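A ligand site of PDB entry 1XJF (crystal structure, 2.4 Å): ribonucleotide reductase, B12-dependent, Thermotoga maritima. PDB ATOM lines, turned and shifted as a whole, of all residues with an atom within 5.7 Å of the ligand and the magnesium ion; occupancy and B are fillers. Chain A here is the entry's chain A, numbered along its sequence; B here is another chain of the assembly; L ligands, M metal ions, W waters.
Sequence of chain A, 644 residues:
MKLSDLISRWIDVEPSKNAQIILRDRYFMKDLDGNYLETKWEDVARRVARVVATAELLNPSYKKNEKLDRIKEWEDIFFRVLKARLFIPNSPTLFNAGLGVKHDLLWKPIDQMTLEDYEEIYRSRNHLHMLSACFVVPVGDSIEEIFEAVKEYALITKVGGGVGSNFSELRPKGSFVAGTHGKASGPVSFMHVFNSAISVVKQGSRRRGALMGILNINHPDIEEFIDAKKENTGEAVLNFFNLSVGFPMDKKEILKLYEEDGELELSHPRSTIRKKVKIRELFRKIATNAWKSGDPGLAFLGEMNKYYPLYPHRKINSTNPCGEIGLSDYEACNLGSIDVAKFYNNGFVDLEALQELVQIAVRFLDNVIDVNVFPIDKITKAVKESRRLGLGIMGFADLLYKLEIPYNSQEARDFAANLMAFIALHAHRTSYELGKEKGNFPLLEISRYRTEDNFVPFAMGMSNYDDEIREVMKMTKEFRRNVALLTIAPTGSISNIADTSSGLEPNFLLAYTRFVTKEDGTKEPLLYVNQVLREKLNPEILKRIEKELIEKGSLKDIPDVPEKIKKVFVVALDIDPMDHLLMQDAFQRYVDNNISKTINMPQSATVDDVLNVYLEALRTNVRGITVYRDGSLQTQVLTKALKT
An oxygen (O1) of the ligand lies within salt-bridge range of the guanidinium group (NH1) of Arg 171, at 2.7 Å. The backbone NH (N) of Gly 179 is in hydrogen-bond range of an oxygen (O6) of the ligand, 3.1 Å away. A nitrogen (N5) of the ligand lies within hydrogen-bond range of the backbone NH of Ser 185 (3.1 Å). N2 of the ligand is in hydrogen-bond range of OG1 of Thr 180, at 3.0 Å. The side-chain amino group (NZ) of Lys 158 of chain B is in salt-bridge range of an oxygen (O4) of the ligand (3.2 Å). The backbone NH (N) of Ile 143 is in hydrogen-bond range of an oxygen (O8) of the ligand (2.8 Å). The backbone NH of Ala 178 lies within hydrogen-bond range of an oxygen (O1) of the ligand, at 2.8 Å. The backbone carbonyl oxygen of Lys 202 of chain B is in hydrogen-bond range of a nitrogen (N3) of the ligand, at 2.6 Å. The backbone NH of Lys 202 of chain B lies within hydrogen-bond range of a nitrogen (N4) of the ligand (3.0 Å). OD1 of Asp 141 sits at hydrogen-bond distance from O12 of the ligand, 3.0 Å away.
O of Phe 176 lies within hydrogen-bond range of NH1 of Arg 171 (3.0 Å). OG of Ser 185 sits at hydrogen-bond distance from O of Val 200 of chain B. OD2 of Asp 141 is in salt-bridge range of NE of Arg 171 (2.7 Å).
Ser 142 touches the ligand. Ile 146 touches the ligand (CD1 to C4, 3.6 Å). Val 177 touches the ligand. Lys 183 touches the ligand. Ala 184 touches the ligand (CA to N5, 3.2 Å). Phe 190 touches the ligand. Val 200 of chain B touches the ligand. CG1 of Val 201 of chain B touches N3 of the ligand (3.6 Å). Hydrophobic or aromatic side chains that line the ligand: Ile 143, Ile 146, Val 177, Ala 178, Ala 184, Phe 190 and Val 201 of chain B. Of the 25 residues printed, 17 come within 4 Å of the ligand.
Ser 142 touches the magnesium ion (CB to MG, 3.9 Å). Of the 25 residues printed, 1 comes within 4 Å of the magnesium ion. The nearest printed residue that does not touch the magnesium ion is Asp 141 (4.3 Å).
The magnesium ion is bound by an oxygen (O5) of the ligand and an oxygen (O7) of the ligand.
Water W2 lies within hydrogen-bond range of O of Arg 171 (2.8 Å), O12 of the ligand (2.8 Å) and N of Gly 186 (2.8 Å). Water W1 lies within hydrogen-bond range of the backbone NH of Glu 144 (2.8 Å), an oxygen (O8) of the ligand (3.1 Å) and the backbone NH of Ile 143 (3.4 Å).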
ATOM      1  N   GLY A 140      10.070  10.643  27.761  1.00  0.00           N
ATOM      2  CA  GLY A 140      10.625  11.550  26.731  1.00  0.00           C
ATOM      3  C   GLY A 140       9.626  12.306  25.858  1.00  0.00           C
ATOM      4  O   GLY A 140       8.420  11.994  25.839  1.00  0.00           O
ATOM      5  N   ASP A 141      10.150  13.286  25.097  1.00  0.00           N
ATOM      6  CA  ASP A 141       9.358  14.170  24.251  1.00  0.00           C
ATOM      7  C   ASP A 141       9.041  13.631  22.836  1.00  0.00           C
ATOM      8  O   ASP A 141       9.267  14.365  21.841  1.00  0.00           O
ATOM      9  CB  ASP A 141      10.058  15.538  24.119  1.00  0.00           C
ATOM     10  CG  ASP A 141       9.080  16.659  23.778  1.00  0.00           C
ATOM     11  OD1 ASP A 141       7.926  16.511  24.154  1.00  0.00           O
ATOM     12  OD2 ASP A 141       9.438  17.703  23.148  1.00  0.00           O
ATOM     13  N   SER A 142       8.547  12.395  22.737  1.00  0.00           N
ATOM     14  CA  SER A 142       8.160  11.825  21.432  1.00  0.00           C
ATOM     15  C   SER A 142       6.964  10.962  21.606  1.00  0.00           C
ATOM     16  O   SER A 142       6.724  10.470  22.713  1.00  0.00           O
ATOM     17  CB  SER A 142       9.305  11.057  20.766  1.00  0.00           C
ATOM     18  OG  SER A 142       9.850  10.062  21.601  1.00  0.00           O
ATOM     19  N   ILE A 143       6.153  10.797  20.548  1.00  0.00           N
ATOM     20  CA  ILE A 143       4.995   9.904  20.583  1.00  0.00           C
ATOM     21  C   ILE A 143       5.449   8.483  20.948  1.00  0.00           C
ATOM     22  O   ILE A 143       4.874   7.845  21.813  1.00  0.00           O
ATOM     23  CB  ILE A 143       4.206   9.906  19.229  1.00  0.00           C
ATOM     24  CG1 ILE A 143       3.454  11.218  18.976  1.00  0.00           C
ATOM     25  CG2 ILE A 143       3.225   8.772  19.172  1.00  0.00           C
ATOM     26  CD1 ILE A 143       2.265  11.507  19.826  1.00  0.00           C
ATOM     27  N   GLU A 144       6.511   8.002  20.296  1.00  0.00           N
ATOM     28  CA  GLU A 144       7.149   6.716  20.620  1.00  0.00           C
ATOM     29  C   GLU A 144       7.464   6.541  22.110  1.00  0.00           C
ATOM     30  O   GLU A 144       7.186   5.487  22.695  1.00  0.00           O
ATOM     31  CB  GLU A 144       8.418   6.552  19.777  1.00  0.00           C
ATOM     32  CG  GLU A 144       9.434   5.523  20.301  1.00  0.00           C
ATOM     33  CD  GLU A 144       8.985   4.079  20.093  1.00  0.00           C
ATOM     34  OE1 GLU A 144       8.350   3.845  19.032  1.00  0.00           O
ATOM     35  OE2 GLU A 144       9.240   3.208  20.978  1.00  0.00           O
ATOM     36  N   ILE A 146       6.445   8.446  24.829  1.00  0.00           N
ATOM     37  CA  ILE A 146       5.250   8.579  25.607  1.00  0.00           C
ATOM     38  C   ILE A 146       4.448   7.291  25.701  1.00  0.00           C
ATOM     39  O   ILE A 146       4.049   6.868  26.787  1.00  0.00           O
ATOM     40  CB  ILE A 146       4.310   9.661  25.016  1.00  0.00           C
ATOM     41  CG1 ILE A 146       5.022  11.030  25.048  1.00  0.00           C
ATOM     42  CG2 ILE A 146       2.988   9.656  25.771  1.00  0.00           C
ATOM     43  CD1 ILE A 146       4.388  12.121  24.265  1.00  0.00           C
ATOM     44  N   LEU A 170       7.866  16.830  28.128  1.00  0.00           N
ATOM     45  CA  LEU A 170       6.839  16.942  27.142  1.00  0.00           C
ATOM     46  C   LEU A 170       6.640  18.397  26.816  1.00  0.00           C
ATOM     47  O   LEU A 170       6.433  19.197  27.712  1.00  0.00           O
ATOM     48  CB  LEU A 170       5.540  16.284  27.624  1.00  0.00           C
ATOM     49  CG  LEU A 170       5.546  14.771  27.890  1.00  0.00           C
ATOM     50  CD1 LEU A 170       4.109  14.311  27.775  1.00  0.00           C
ATOM     51  CD2 LEU A 170       6.458  13.975  26.984  1.00  0.00           C
ATOM     52  N   ARG A 171       6.735  18.729  25.527  1.00  0.00           N
ATOM     53  CA  ARG A 171       6.754  20.126  25.083  1.00  0.00           C
ATOM     54  C   ARG A 171       5.354  20.721  25.314  1.00  0.00           C
ATOM     55  O   ARG A 171       4.377  20.019  25.274  1.00  0.00           O
ATOM     56  CB  ARG A 171       7.245  20.217  23.631  1.00  0.00           C
ATOM     57  CG  ARG A 171       6.215  19.925  22.505  1.00  0.00           C
ATOM     58  CD  ARG A 171       6.866  19.792  21.133  1.00  0.00           C
ATOM     59  NE  ARG A 171       8.054  18.895  21.182  1.00  0.00           N
ATOM     60  CZ  ARG A 171       8.739  18.565  20.089  1.00  0.00           C
ATOM     61  NH1 ARG A 171       8.324  19.008  18.919  1.00  0.00           N
ATOM     62  NH2 ARG A 171       9.797  17.764  20.133  1.00  0.00           N
ATOM     63  N   PHE A 176       5.044  23.588  18.171  1.00  0.00           N
ATOM     64  CA  PHE A 176       5.345  23.035  16.832  1.00  0.00           C
ATOM     65  C   PHE A 176       5.832  21.582  16.855  1.00  0.00           C
ATOM     66  O   PHE A 176       6.688  21.227  17.676  1.00  0.00           O
ATOM     67  CB  PHE A 176       6.424  23.883  16.128  1.00  0.00           C
ATOM     68  CG  PHE A 176       6.937  23.275  14.858  1.00  0.00           C
ATOM     69  CD1 PHE A 176       6.143  23.279  13.717  1.00  0.00           C
ATOM     70  CD2 PHE A 176       8.187  22.651  14.819  1.00  0.00           C
ATOM     71  CE1 PHE A 176       6.582  22.688  12.536  1.00  0.00           C
ATOM     72  CE2 PHE A 176       8.654  22.052  13.642  1.00  0.00           C
ATOM     73  CZ  PHE A 176       7.849  22.077  12.497  1.00  0.00           C
ATOM     74  N   VAL A 177       5.350  20.749  15.920  1.00  0.00           N
ATOM     75  CA  VAL A 177       5.938  19.390  15.737  1.00  0.00           C
ATOM     76  C   VAL A 177       6.368  19.080  14.310  1.00  0.00           C
ATOM     77  O   VAL A 177       5.559  19.129  13.389  1.00  0.00           O
ATOM     78  CB  VAL A 177       4.985  18.196  16.248  1.00  0.00           C
ATOM     79  CG1 VAL A 177       5.723  16.847  16.253  1.00  0.00           C
ATOM     80  CG2 VAL A 177       4.404  18.511  17.611  1.00  0.00           C
ATOM     81  N   ALA A 178       7.638  18.723  14.138  1.00  0.00           N
ATOM     82  CA  ALA A 178       8.216  18.479  12.791  1.00  0.00           C
ATOM     83  C   ALA A 178       7.543  17.294  12.109  1.00  0.00           C
ATOM     84  O   ALA A 178       7.190  17.360  10.937  1.00  0.00           O
ATOM     85  CB  ALA A 178       9.775  18.291  12.833  1.00  0.00           C
ATOM     86  N   GLY A 179       7.340  16.218  12.861  1.00  0.00           N
ATOM     87  CA  GLY A 179       6.827  14.972  12.285  1.00  0.00           C
ATOM     88  C   GLY A 179       5.299  14.727  12.201  1.00  0.00           C
ATOM     89  O   GLY A 179       4.893  13.551  12.016  1.00  0.00           O
ATOM     90  N   THR A 180       4.469  15.776  12.317  1.00  0.00           N
ATOM     91  CA  THR A 180       2.974  15.643  12.224  1.00  0.00           C
ATOM     92  C   THR A 180       2.317  16.899  11.681  1.00  0.00           C
ATOM     93  O   THR A 180       2.977  17.944  11.609  1.00  0.00           O
ATOM     94  CB  THR A 180       2.216  15.504  13.620  1.00  0.00           C
ATOM     95  OG1 THR A 180       3.123  15.276  14.701  1.00  0.00           O
ATOM     96  CG2 THR A 180       1.133  14.445  13.587  1.00  0.00           C
ATOM     97  N   GLY A 182      -0.295  17.748  13.441  1.00  0.00           N
ATOM     98  CA  GLY A 182      -0.802  18.187  14.753  1.00  0.00           C
ATOM     99  C   GLY A 182       0.151  19.122  15.502  1.00  0.00           C
ATOM    100  O   GLY A 182       1.374  19.092  15.270  1.00  0.00           O
ATOM    101  N   LYS A 183      -0.430  19.963  16.358  1.00  0.00           N
ATOM    102  CA  LYS A 183       0.267  20.670  17.469  1.00  0.00           C
ATOM    103  C   LYS A 183       0.375  19.700  18.653  1.00  0.00           C
ATOM    104  O   LYS A 183      -0.614  18.994  18.951  1.00  0.00           O
ATOM    105  CB  LYS A 183      -0.556  21.877  17.951  1.00  0.00           C
ATOM    106  CG  LYS A 183      -0.921  22.907  16.903  1.00  0.00           C
ATOM    107  CD  LYS A 183       0.116  24.002  16.785  1.00  0.00           C
ATOM    108  CE  LYS A 183      -0.111  24.877  15.561  1.00  0.00           C
ATOM    109  NZ  LYS A 183      -1.486  25.520  15.568  1.00  0.00           N
ATOM    110  N   ALA A 184       1.520  19.687  19.348  1.00  0.00           N
ATOM    111  CA  ALA A 184       1.701  18.835  20.542  1.00  0.00           C
ATOM    112  C   ALA A 184       0.621  19.114  21.560  1.00  0.00           C
ATOM    113  O   ALA A 184       0.269  20.260  21.780  1.00  0.00           O
ATOM    114  CB  ALA A 184       3.039  19.048  21.141  1.00  0.00           C
ATOM    115  N   SER A 185       0.078  18.056  22.162  1.00  0.00           N
ATOM    116  CA  SER A 185      -1.013  18.180  23.172  1.00  0.00           C
ATOM    117  C   SER A 185      -0.558  18.727  24.538  1.00  0.00           C
ATOM    118  O   SER A 185      -1.349  19.348  25.258  1.00  0.00           O
ATOM    119  CB  SER A 185      -1.741  16.848  23.373  1.00  0.00           C
ATOM    120  OG  SER A 185      -2.497  16.455  22.235  1.00  0.00           O
ATOM    121  N   GLY A 186       0.699  18.467  24.892  1.00  0.00           N
ATOM    122  CA  GLY A 186       1.239  18.933  26.173  1.00  0.00           C
ATOM    123  C   GLY A 186       1.062  17.937  27.312  1.00  0.00           C
ATOM    124  O   GLY A 186       0.188  17.054  27.244  1.00  0.00           O
ATOM    125  N   PHE A 190      -1.662  14.505  27.793  1.00  0.00           N
ATOM    126  CA  PHE A 190      -1.167  13.135  27.652  1.00  0.00           C
ATOM    127  C   PHE A 190      -1.278  12.343  28.933  1.00  0.00           C
ATOM    128  O   PHE A 190      -1.412  11.137  28.873  1.00  0.00           O
ATOM    129  CB  PHE A 190       0.299  13.130  27.211  1.00  0.00           C
ATOM    130  CG  PHE A 190       0.489  13.366  25.755  1.00  0.00           C
ATOM    131  CD1 PHE A 190       0.027  12.440  24.817  1.00  0.00           C
ATOM    132  CD2 PHE A 190       1.118  14.529  25.303  1.00  0.00           C
ATOM    133  CE1 PHE A 190       0.205  12.677  23.443  1.00  0.00           C
ATOM    134  CE2 PHE A 190       1.302  14.759  23.949  1.00  0.00           C
ATOM    135  CZ  PHE A 190       0.846  13.854  23.007  1.00  0.00           C
ATOM    136  N   THR B 157      -1.901   7.116  13.806  1.00  0.00           N
ATOM    137  CA  THR B 157      -2.743   8.299  13.836  1.00  0.00           C
ATOM    138  C   THR B 157      -1.931   9.571  13.660  1.00  0.00           C
ATOM    139  O   THR B 157      -2.378  10.558  13.048  1.00  0.00           O
ATOM    140  CB  THR B 157      -3.518   8.351  15.160  1.00  0.00           C
ATOM    141  OG1 THR B 157      -4.287   7.154  15.258  1.00  0.00           O
ATOM    142  CG2 THR B 157      -4.476   9.552  15.222  1.00  0.00           C
ATOM    143  N   LYS B 158      -0.707   9.525  14.175  1.00  0.00           N
ATOM    144  CA  LYS B 158       0.243  10.609  13.984  1.00  0.00           C
ATOM    145  C   LYS B 158       0.545  10.904  12.499  1.00  0.00           C
ATOM    146  O   LYS B 158       0.751  12.047  12.125  1.00  0.00           O
ATOM    147  CB  LYS B 158       1.533  10.266  14.731  1.00  0.00           C
ATOM    148  CG  LYS B 158       2.538  11.406  14.833  1.00  0.00           C
ATOM    149  CD  LYS B 158       3.910  10.815  15.050  1.00  0.00           C
ATOM    150  CE  LYS B 158       4.986  11.867  15.014  1.00  0.00           C
ATOM    151  NZ  LYS B 158       6.327  11.204  14.922  1.00  0.00           N
ATOM    152  N   VAL B 200      -6.038  12.303  22.132  1.00  0.00           N
ATOM    153  CA  VAL B 200      -4.861  13.080  22.535  1.00  0.00           C
ATOM    154  C   VAL B 200      -3.863  13.276  21.363  1.00  0.00           C
ATOM    155  O   VAL B 200      -3.146  14.290  21.324  1.00  0.00           O
ATOM    156  CB  VAL B 200      -4.218  12.374  23.796  1.00  0.00           C
ATOM    157  CG1 VAL B 200      -2.748  12.138  23.655  1.00  0.00           C
ATOM    158  CG2 VAL B 200      -4.582  13.105  25.073  1.00  0.00           C
ATOM    159  N   VAL B 201      -3.830  12.304  20.440  1.00  0.00           N
ATOM    160  CA  VAL B 201      -3.085  12.374  19.176  1.00  0.00           C
ATOM    161  C   VAL B 201      -3.934  12.960  18.022  1.00  0.00           C
ATOM    162  O   VAL B 201      -4.762  12.297  17.397  1.00  0.00           O
ATOM    163  CB  VAL B 201      -2.493  11.006  18.769  1.00  0.00           C
ATOM    164  CG1 VAL B 201      -1.589  11.169  17.577  1.00  0.00           C
ATOM    165  CG2 VAL B 201      -1.683  10.442  19.902  1.00  0.00           C
ATOM    166  N   LYS B 202      -3.671  14.236  17.757  1.00  0.00           N
ATOM    167  CA  LYS B 202      -4.476  15.057  16.883  1.00  0.00           C
ATOM    168  C   LYS B 202      -3.809  15.234  15.492  1.00  0.00           C
ATOM    169  O   LYS B 202      -2.578  15.098  15.339  1.00  0.00           O
ATOM    170  CB  LYS B 202      -4.717  16.394  17.579  1.00  0.00           C
ATOM    171  CG  LYS B 202      -6.186  16.828  17.637  1.00  0.00           C
ATOM    172  CD  LYS B 202      -6.442  17.682  18.888  1.00  0.00           C
ATOM    173  CE  LYS B 202      -6.701  16.810  20.112  1.00  0.00           C
ATOM    174  NZ  LYS B 202      -6.551  17.551  21.404  1.00  0.00           N
ATOM    175  N   GLN B 203      -4.645  15.531  14.483  1.00  0.00           N
ATOM    176  CA  GLN B 203      -4.209  15.532  13.069  1.00  0.00           C
ATOM    177  C   GLN B 203      -4.441  16.864  12.349  1.00  0.00           C
ATOM    178  O   GLN B 203      -3.853  17.090  11.259  1.00  0.00           O
ATOM    179  CB  GLN B 203      -4.914  14.418  12.313  1.00  0.00           C
ATOM    180  CG  GLN B 203      -4.180  13.084  12.334  1.00  0.00           C
ATOM    181  CD  GLN B 203      -5.118  11.871  12.355  1.00  0.00           C
ATOM    182  OE1 GLN B 203      -4.911  10.896  11.628  1.00  0.00           O
ATOM    183  NE2 GLN B 203      -6.137  11.914  13.190  1.00  0.00           N
HETATM  184  P1  LIG L   1       9.893  16.802  16.283  1.00  0.00           P
HETATM  185  O1  LIG L   1       9.136  18.280  16.440  1.00  0.00           O
HETATM  186  O2  LIG L   1      10.290  16.170  17.769  1.00  0.00           O
HETATM  187  O3  LIG L   1      11.128  16.815  15.467  1.00  0.00           O
HETATM  188  P2  LIG L   1       8.684  14.293  15.850  1.00  0.00           P
HETATM  189  O4  LIG L   1       8.437  13.611  14.541  1.00  0.00           O
HETATM  190  O5  LIG L   1       9.849  13.870  16.695  1.00  0.00           O
HETATM  191  O6  LIG L   1       8.709  15.882  15.588  1.00  0.00           O
HETATM  192  P3  LIG L   1       7.293  13.356  18.221  1.00  0.00           P
HETATM  193  O7  LIG L   1       8.706  13.410  18.641  1.00  0.00           O
HETATM  194  O8  LIG L   1       6.589  12.050  18.136  1.00  0.00           O
HETATM  195  O9  LIG L   1       7.296  14.193  16.785  1.00  0.00           O
HETATM  196  O10 LIG L   1       6.395  14.378  19.085  1.00  0.00           O
HETATM  197  C1  LIG L   1       7.065  15.134  20.069  1.00  0.00           C
HETATM  198  C2  LIG L   1       6.069  15.842  20.947  1.00  0.00           C
HETATM  199  O11 LIG L   1       4.922  16.279  20.200  1.00  0.00           O
HETATM  200  C3  LIG L   1       5.510  14.958  22.079  1.00  0.00           C
HETATM  201  O12 LIG L   1       5.150  15.821  23.171  1.00  0.00           O
HETATM  202  C4  LIG L   1       4.235  14.403  21.515  1.00  0.00           C
HETATM  203  C5  LIG L   1       3.724  15.531  20.634  1.00  0.00           C
HETATM  204  N1  LIG L   1       2.891  15.105  19.427  1.00  0.00           N
HETATM  205  C6  LIG L   1       3.359  14.499  18.287  1.00  0.00           C
HETATM  206  N2  LIG L   1       2.327  14.308  17.447  1.00  0.00           N
HETATM  207  C7  LIG L   1       1.230  14.776  18.026  1.00  0.00           C
HETATM  208  C8  LIG L   1      -0.079  14.860  17.620  1.00  0.00           C
HETATM  209  N3  LIG L   1      -0.388  14.380  16.433  1.00  0.00           N
HETATM  210  N4  LIG L   1      -1.023  15.402  18.398  1.00  0.00           N
HETATM  211  C9  LIG L   1      -0.657  15.880  19.593  1.00  0.00           C
HETATM  212  N5  LIG L   1       0.625  15.839  20.031  1.00  0.00           N
HETATM  213  C10 LIG L   1       1.575  15.291  19.274  1.00  0.00           C
HETATM  214 MG    MG M   1      10.882  13.230  18.000  1.00  0.00          MG
HETATM  215  O   HOH W   1       7.437   9.040  17.901  1.00  0.00           O
HETATM  216  O   HOH W   2       3.355  17.620  24.328  1.00  0.00           O
